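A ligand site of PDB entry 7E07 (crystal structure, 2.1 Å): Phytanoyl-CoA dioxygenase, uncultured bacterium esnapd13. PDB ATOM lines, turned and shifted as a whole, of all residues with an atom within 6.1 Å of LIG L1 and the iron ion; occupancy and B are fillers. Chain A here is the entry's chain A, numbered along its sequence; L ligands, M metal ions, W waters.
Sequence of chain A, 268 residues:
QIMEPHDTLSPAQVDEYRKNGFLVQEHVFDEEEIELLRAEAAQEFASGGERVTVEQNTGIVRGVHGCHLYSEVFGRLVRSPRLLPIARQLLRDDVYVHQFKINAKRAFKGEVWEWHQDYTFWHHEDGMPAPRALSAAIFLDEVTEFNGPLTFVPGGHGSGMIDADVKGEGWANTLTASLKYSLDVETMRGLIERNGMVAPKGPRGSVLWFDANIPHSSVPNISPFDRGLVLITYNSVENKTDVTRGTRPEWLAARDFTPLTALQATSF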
ATOM      1  N   GLN A  99       3.284  23.922  11.237  1.00  0.00           N
ATOM      2  CA  GLN A  99       3.706  22.612  11.710  1.00  0.00           C
ATOM      3  C   GLN A  99       4.806  22.760  12.699  1.00  0.00           C
ATOM      4  O   GLN A  99       5.595  23.724  12.659  1.00  0.00           O
ATOM      5  CB  GLN A  99       4.190  21.798  10.464  1.00  0.00           C
ATOM      6  CG  GLN A  99       4.721  20.408  10.665  1.00  0.00           C
ATOM      7  CD  GLN A  99       5.059  19.749   9.326  1.00  0.00           C
ATOM      8  OE1 GLN A  99       6.221  19.649   8.956  1.00  0.00           O
ATOM      9  NE2 GLN A  99       4.045  19.314   8.590  1.00  0.00           N
ATOM     10  N   LYS A 101       7.561  20.075  14.659  1.00  0.00           N
ATOM     11  CA  LYS A 101       8.063  18.706  14.905  1.00  0.00           C
ATOM     12  C   LYS A 101       9.422  18.689  15.548  1.00  0.00           C
ATOM     13  O   LYS A 101      10.218  19.648  15.433  1.00  0.00           O
ATOM     14  CB  LYS A 101       8.007  17.883  13.599  1.00  0.00           C
ATOM     15  CG  LYS A 101       9.004  18.372  12.551  1.00  0.00           C
ATOM     16  CD  LYS A 101       8.660  17.926  11.121  1.00  0.00           C
ATOM     17  CE  LYS A 101       9.398  18.750  10.067  1.00  0.00           C
ATOM     18  NZ  LYS A 101       8.686  20.030   9.653  1.00  0.00           N
ATOM     19  N   ASN A 103      12.663  16.123  15.558  1.00  0.00           N
ATOM     20  CA  ASN A 103      13.342  14.982  14.909  1.00  0.00           C
ATOM     21  C   ASN A 103      14.641  14.664  15.727  1.00  0.00           C
ATOM     22  O   ASN A 103      15.540  15.553  15.823  1.00  0.00           O
ATOM     23  CB  ASN A 103      13.709  15.328  13.441  1.00  0.00           C
ATOM     24  CG  ASN A 103      12.483  15.301  12.503  1.00  0.00           C
ATOM     25  OD1 ASN A 103      11.396  14.929  12.922  1.00  0.00           O
ATOM     26  ND2 ASN A 103      12.674  15.698  11.257  1.00  0.00           N
ATOM     27  N   LYS A 105      17.858  12.440  16.091  1.00  0.00           N
ATOM     28  CA  LYS A 105      18.786  11.663  15.234  1.00  0.00           C
ATOM     29  C   LYS A 105      19.785  11.179  16.232  1.00  0.00           C
ATOM     30  O   LYS A 105      20.735  11.895  16.601  1.00  0.00           O
ATOM     31  CB  LYS A 105      19.291  12.610  14.146  1.00  0.00           C
ATOM     32  CG  LYS A 105      20.128  11.981  13.058  1.00  0.00           C
ATOM     33  CD  LYS A 105      20.065  12.772  11.782  1.00  0.00           C
ATOM     34  CE  LYS A 105      19.246  12.069  10.742  1.00  0.00           C
ATOM     35  NZ  LYS A 105      19.498  12.660   9.412  1.00  0.00           N
ATOM     36  N   TRP A 113      17.158  10.912   5.341  1.00  0.00           N
ATOM     37  CA  TRP A 113      16.009  11.664   4.749  1.00  0.00           C
ATOM     38  C   TRP A 113      16.342  12.062   3.334  1.00  0.00           C
ATOM     39  O   TRP A 113      17.254  12.830   3.111  1.00  0.00           O
ATOM     40  CB  TRP A 113      15.686  12.908   5.562  1.00  0.00           C
ATOM     41  CG  TRP A 113      15.117  12.661   6.933  1.00  0.00           C
ATOM     42  CD1 TRP A 113      15.821  12.239   8.030  1.00  0.00           C
ATOM     43  CD2 TRP A 113      13.752  12.816   7.372  1.00  0.00           C
ATOM     44  NE1 TRP A 113      14.970  12.109   9.129  1.00  0.00           N
ATOM     45  CE2 TRP A 113      13.706  12.468   8.755  1.00  0.00           C
ATOM     46  CE3 TRP A 113      12.562  13.210   6.747  1.00  0.00           C
ATOM     47  CZ2 TRP A 113      12.500  12.518   9.507  1.00  0.00           C
ATOM     48  CZ3 TRP A 113      11.350  13.203   7.499  1.00  0.00           C
ATOM     49  CH2 TRP A 113      11.346  12.868   8.859  1.00  0.00           C
ATOM     50  N   HIS A 116      14.284  16.610  -0.659  1.00  0.00           N
ATOM     51  CA  HIS A 116      12.902  17.073  -0.741  1.00  0.00           C
ATOM     52  C   HIS A 116      12.794  18.566  -0.448  1.00  0.00           C
ATOM     53  O   HIS A 116      13.756  19.237   0.024  1.00  0.00           O
ATOM     54  CB  HIS A 116      11.970  16.262   0.163  1.00  0.00           C
ATOM     55  CG  HIS A 116      12.145  16.526   1.616  1.00  0.00           C
ATOM     56  ND1 HIS A 116      13.147  15.954   2.359  1.00  0.00           N
ATOM     57  CD2 HIS A 116      11.454  17.330   2.465  1.00  0.00           C
ATOM     58  CE1 HIS A 116      13.087  16.404   3.598  1.00  0.00           C
ATOM     59  NE2 HIS A 116      12.060  17.227   3.687  1.00  0.00           N
ATOM     60  N   GLN A 117      11.659  19.112  -0.893  1.00  0.00           N
ATOM     61  CA  GLN A 117      11.258  20.480  -0.619  1.00  0.00           C
ATOM     62  C   GLN A 117      10.053  20.361   0.297  1.00  0.00           C
ATOM     63  O   GLN A 117       9.109  19.578   0.008  1.00  0.00           O
ATOM     64  CB  GLN A 117      10.925  21.209  -1.882  1.00  0.00           C
ATOM     65  CG  GLN A 117      12.123  21.492  -2.702  1.00  0.00           C
ATOM     66  CD  GLN A 117      11.731  21.984  -4.094  1.00  0.00           C
ATOM     67  OE1 GLN A 117      11.103  21.232  -4.839  1.00  0.00           O
ATOM     68  NE2 GLN A 117      12.091  23.219  -4.458  1.00  0.00           N
ATOM     69  N   ASP A 118      10.084  21.018   1.449  1.00  0.00           N
ATOM     70  CA  ASP A 118       8.950  20.889   2.402  1.00  0.00           C
ATOM     71  C   ASP A 118       7.639  21.383   1.785  1.00  0.00           C
ATOM     72  O   ASP A 118       6.600  20.870   2.065  1.00  0.00           O
ATOM     73  CB  ASP A 118       9.164  21.709   3.673  1.00  0.00           C
ATOM     74  CG  ASP A 118      10.249  21.143   4.590  1.00  0.00           C
ATOM     75  OD1 ASP A 118      10.625  19.943   4.467  1.00  0.00           O
ATOM     76  OD2 ASP A 118      10.735  21.948   5.426  1.00  0.00           O
ATOM     77  N   GLY A 148      24.760  13.913  11.092  1.00  0.00           N
ATOM     78  CA  GLY A 148      23.642  13.937  10.184  1.00  0.00           C
ATOM     79  C   GLY A 148      23.002  15.312  10.054  1.00  0.00           C
ATOM     80  O   GLY A 148      21.827  15.397  10.222  1.00  0.00           O
ATOM     81  N   PRO A 149      23.787  16.369   9.825  1.00  0.00           N
ATOM     82  CA  PRO A 149      23.236  17.712   9.667  1.00  0.00           C
ATOM     83  C   PRO A 149      22.262  17.825   8.514  1.00  0.00           C
ATOM     84  O   PRO A 149      22.395  17.158   7.482  1.00  0.00           O
ATOM     85  CB  PRO A 149      24.486  18.563   9.352  1.00  0.00           C
ATOM     86  CG  PRO A 149      25.421  17.566   8.666  1.00  0.00           C
ATOM     87  CD  PRO A 149      25.208  16.331   9.464  1.00  0.00           C
ATOM     88  N   LEU A 150      21.308  18.726   8.648  1.00  0.00           N
ATOM     89  CA  LEU A 150      20.532  19.096   7.480  1.00  0.00           C
ATOM     90  C   LEU A 150      21.466  19.641   6.414  1.00  0.00           C
ATOM     91  O   LEU A 150      22.331  20.484   6.699  1.00  0.00           O
ATOM     92  CB  LEU A 150      19.507  20.190   7.866  1.00  0.00           C
ATOM     93  CG  LEU A 150      18.052  19.875   7.975  1.00  0.00           C
ATOM     94  CD1 LEU A 150      17.760  18.396   8.034  1.00  0.00           C
ATOM     95  CD2 LEU A 150      17.499  20.528   9.223  1.00  0.00           C
ATOM     96  N   PHE A 210      15.247  28.216   7.617  1.00  0.00           N
ATOM     97  CA  PHE A 210      15.285  27.810   6.216  1.00  0.00           C
ATOM     98  C   PHE A 210      13.968  27.902   5.476  1.00  0.00           C
ATOM     99  O   PHE A 210      12.898  27.649   6.031  1.00  0.00           O
ATOM    100  CB  PHE A 210      15.940  26.445   6.016  1.00  0.00           C
ATOM    101  CG  PHE A 210      15.208  25.292   6.587  1.00  0.00           C
ATOM    102  CD1 PHE A 210      14.395  24.521   5.817  1.00  0.00           C
ATOM    103  CD2 PHE A 210      15.506  24.828   7.846  1.00  0.00           C
ATOM    104  CE1 PHE A 210      13.825  23.388   6.308  1.00  0.00           C
ATOM    105  CE2 PHE A 210      14.890  23.722   8.372  1.00  0.00           C
ATOM    106  CZ  PHE A 210      14.043  22.993   7.609  1.00  0.00           C
ATOM    107  N   HIS A 216      16.369  19.959   0.639  1.00  0.00           N
ATOM    108  CA  HIS A 216      17.298  19.527   1.688  1.00  0.00           C
ATOM    109  C   HIS A 216      17.267  18.063   1.904  1.00  0.00           C
ATOM    110  O   HIS A 216      16.277  17.324   1.578  1.00  0.00           O
ATOM    111  CB  HIS A 216      17.074  20.285   3.053  1.00  0.00           C
ATOM    112  CG  HIS A 216      15.655  20.215   3.570  1.00  0.00           C
ATOM    113  ND1 HIS A 216      14.655  20.961   3.029  1.00  0.00           N
ATOM    114  CD2 HIS A 216      15.080  19.463   4.531  1.00  0.00           C
ATOM    115  CE1 HIS A 216      13.524  20.699   3.663  1.00  0.00           C
ATOM    116  NE2 HIS A 216      13.742  19.743   4.533  1.00  0.00           N
ATOM    117  N   SER A 217      18.323  17.646   2.573  1.00  0.00           N
ATOM    118  CA  SER A 217      18.523  16.211   2.880  1.00  0.00           C
ATOM    119  C   SER A 217      19.313  15.988   4.173  1.00  0.00           C
ATOM    120  O   SER A 217      19.972  16.904   4.660  1.00  0.00           O
ATOM    121  CB  SER A 217      19.341  15.562   1.726  1.00  0.00           C
ATOM    122  OG  SER A 217      19.268  14.139   1.846  1.00  0.00           O
ATOM    123  N   SER A 218      19.361  14.746   4.629  1.00  0.00           N
ATOM    124  CA  SER A 218      20.358  14.405   5.680  1.00  0.00           C
ATOM    125  C   SER A 218      20.656  12.907   5.788  1.00  0.00           C
ATOM    126  O   SER A 218      19.845  12.095   5.467  1.00  0.00           O
ATOM    127  CB  SER A 218      19.847  14.857   7.044  1.00  0.00           C
ATOM    128  OG  SER A 218      18.687  14.116   7.367  1.00  0.00           O
ATOM    129  N   ARG A 227      21.675  14.355  17.723  1.00  0.00           N
ATOM    130  CA  ARG A 227      21.349  15.578  16.971  1.00  0.00           C
ATOM    131  C   ARG A 227      19.815  15.862  17.049  1.00  0.00           C
ATOM    132  O   ARG A 227      19.130  15.651  16.090  1.00  0.00           O
ATOM    133  CB  ARG A 227      21.859  15.472  15.515  1.00  0.00           C
ATOM    134  CG  ARG A 227      21.737  16.737  14.706  1.00  0.00           C
ATOM    135  CD  ARG A 227      21.064  16.563  13.366  1.00  0.00           C
ATOM    136  NE  ARG A 227      19.662  16.244  13.503  1.00  0.00           N
ATOM    137  CZ  ARG A 227      18.789  16.094  12.496  1.00  0.00           C
ATOM    138  NH1 ARG A 227      19.130  16.228  11.228  1.00  0.00           N
ATOM    139  NH2 ARG A 227      17.543  15.781  12.767  1.00  0.00           N
ATOM    140  N   LEU A 229      16.627  18.221  16.832  1.00  0.00           N
ATOM    141  CA  LEU A 229      16.208  19.461  16.156  1.00  0.00           C
ATOM    142  C   LEU A 229      14.740  19.693  16.578  1.00  0.00           C
ATOM    143  O   LEU A 229      13.892  18.828  16.417  1.00  0.00           O
ATOM    144  CB  LEU A 229      16.307  19.301  14.657  1.00  0.00           C
ATOM    145  CG  LEU A 229      17.724  19.294  14.073  1.00  0.00           C
ATOM    146  CD1 LEU A 229      17.647  19.400  12.592  1.00  0.00           C
ATOM    147  CD2 LEU A 229      18.610  20.456  14.546  1.00  0.00           C
ATOM    148  N   LEU A 231      11.917  21.771  15.103  1.00  0.00           N
ATOM    149  CA  LEU A 231      11.527  22.444  13.877  1.00  0.00           C
ATOM    150  C   LEU A 231      10.131  23.111  13.985  1.00  0.00           C
ATOM    151  O   LEU A 231       9.116  22.414  14.038  1.00  0.00           O
ATOM    152  CB  LEU A 231      11.527  21.454  12.708  1.00  0.00           C
ATOM    153  CG  LEU A 231      12.996  21.089  12.321  1.00  0.00           C
ATOM    154  CD1 LEU A 231      13.236  19.642  12.607  1.00  0.00           C
ATOM    155  CD2 LEU A 231      13.249  21.353  10.837  1.00  0.00           C
HETATM  156  C1  LIG L   1      11.653  17.228   7.580  1.00  0.00           C
HETATM  157  O1  LIG L   1      10.937  17.782   6.660  1.00  0.00           O
HETATM  158  O2  LIG L   1      11.179  16.585   8.570  1.00  0.00           O
HETATM  159  C2  LIG L   1      13.124  17.327   7.448  1.00  0.00           C
HETATM  160  O3  LIG L   1      13.592  17.744   6.433  1.00  0.00           O
HETATM  161  C3  LIG L   1      14.074  17.109   8.587  1.00  0.00           C
HETATM  162  C4  LIG L   1      15.056  15.949   8.426  1.00  0.00           C
HETATM  163  C5  LIG L   1      16.064  15.855   9.565  1.00  0.00           C
HETATM  164  O4  LIG L   1      17.279  15.599   9.314  1.00  0.00           O
HETATM  165  O5  LIG L   1      15.673  16.007  10.770  1.00  0.00           O
HETATM  166  N1  LG2 L   2       7.622  15.791   6.204  1.00  0.00           N
HETATM  167  C1  LG2 L   2       6.959  17.090   6.523  1.00  0.00           C
HETATM  168  C2  LG2 L   2       5.481  17.071   6.136  1.00  0.00           C
HETATM  169  O1  LG2 L   2       4.830  18.099   6.160  1.00  0.00           O
HETATM  170  C3  LG2 L   2       7.716  18.103   5.667  1.00  0.00           C
HETATM  171  C4  LG2 L   2       8.386  17.281   4.580  1.00  0.00           C
HETATM  172  C5  LG2 L   2       8.691  15.951   5.194  1.00  0.00           C
HETATM  173  O2  LG2 L   2       4.920  16.036   5.782  1.00  0.00           O
HETATM  174 FE    FE M   1      12.077  18.739   5.402  1.00  0.00          FE
HETATM  175  O   HOH W   1       8.562  15.525   8.677  1.00  0.00           O
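ND2 of Asn 103 lies within hydrogen-bond range of O5 of LIG L1, 3.1 Å away. An oxygen (O1) of LG2 L2 is in hydrogen-bond range of the side-chain amide nitrogen (NE2) of Gln 99, at 2.8 Å. The side-chain hydroxyl (OG) of Ser 218 sits at hydrogen-bond distance from an oxygen (O4) of LIG L1 (2.8 Å). O4 of LIG L1 lies within salt-bridge range of NH1 of Arg 227 (2.7 Å). NZ of Lys 105 is in salt-bridge range of O4 of LIG L1 (3.7 Å).
NZ of Lys 101 is in hydrogen-bond range of OE1 of Gln 99 (2.6 Å). The backbone carbonyl oxygen (O) of Lys 101 is in hydrogen-bond range of the backbone NH (N) of Leu 231, 2.7 Å away. The side-chain amino group (NZ) of Lys 105 is in hydrogen-bond range of the side-chain hydroxyl (OG) of Ser 218. The backbone NH of Leu 229 lies within hydrogen-bond range of the backbone carbonyl oxygen of Asn 103 (3.1 Å). The backbone NH (N) of Trp 113 sits at hydrogen-bond distance from the backbone carbonyl oxygen (O) of Ser 218 (2.9 Å). The backbone carbonyl oxygen of Trp 113 sits at hydrogen-bond distance from the side-chain hydroxyl of Ser 217 (2.7 Å). The guanidinium group (NH1) of Arg 227 is in hydrogen-bond range of the backbone carbonyl oxygen (O) of Gly 148 (3.0 Å). O of Lys 105 lies within hydrogen-bond range of N of Arg 227 (2.9 Å).
CE of Lys 101 touches O2 of LIG L1, 3.2 Å away. Trp 113 touches LIG L1. Leu 150 touches LIG L1 (CD1 to O4, 3.1 Å). Hydrophobic or aromatic side chains that line LIG L1: Trp 113, His 116, Leu 150 and His 216. Ten residues have an atom within 4 Å of LIG L1: Lys 101, Asn 103, Lys 105, Trp 113, His 116, Asp 118, Leu 150, His 216, Ser 218 and Arg 227. Along chain A the residues within 4 Å of LIG L1 span positions 101 to 227. The nearest printed residue that does not touch LIG L1 is Leu 229 (4.3 Å).
The iron ion is bound by O1 of LIG L1 (1.9 Å), O3 of LIG L1 (2.1 Å), OD1 of Asp 118 (2.1 Å), NE2 of His 216 (2.1 Å) and NE2 of His 116 (2.3 Å).
Water W1 lies within hydrogen-bond range of N1 of LG2 L2 (2.7 Å) and O2 of LIG L1 (2.8 Å).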
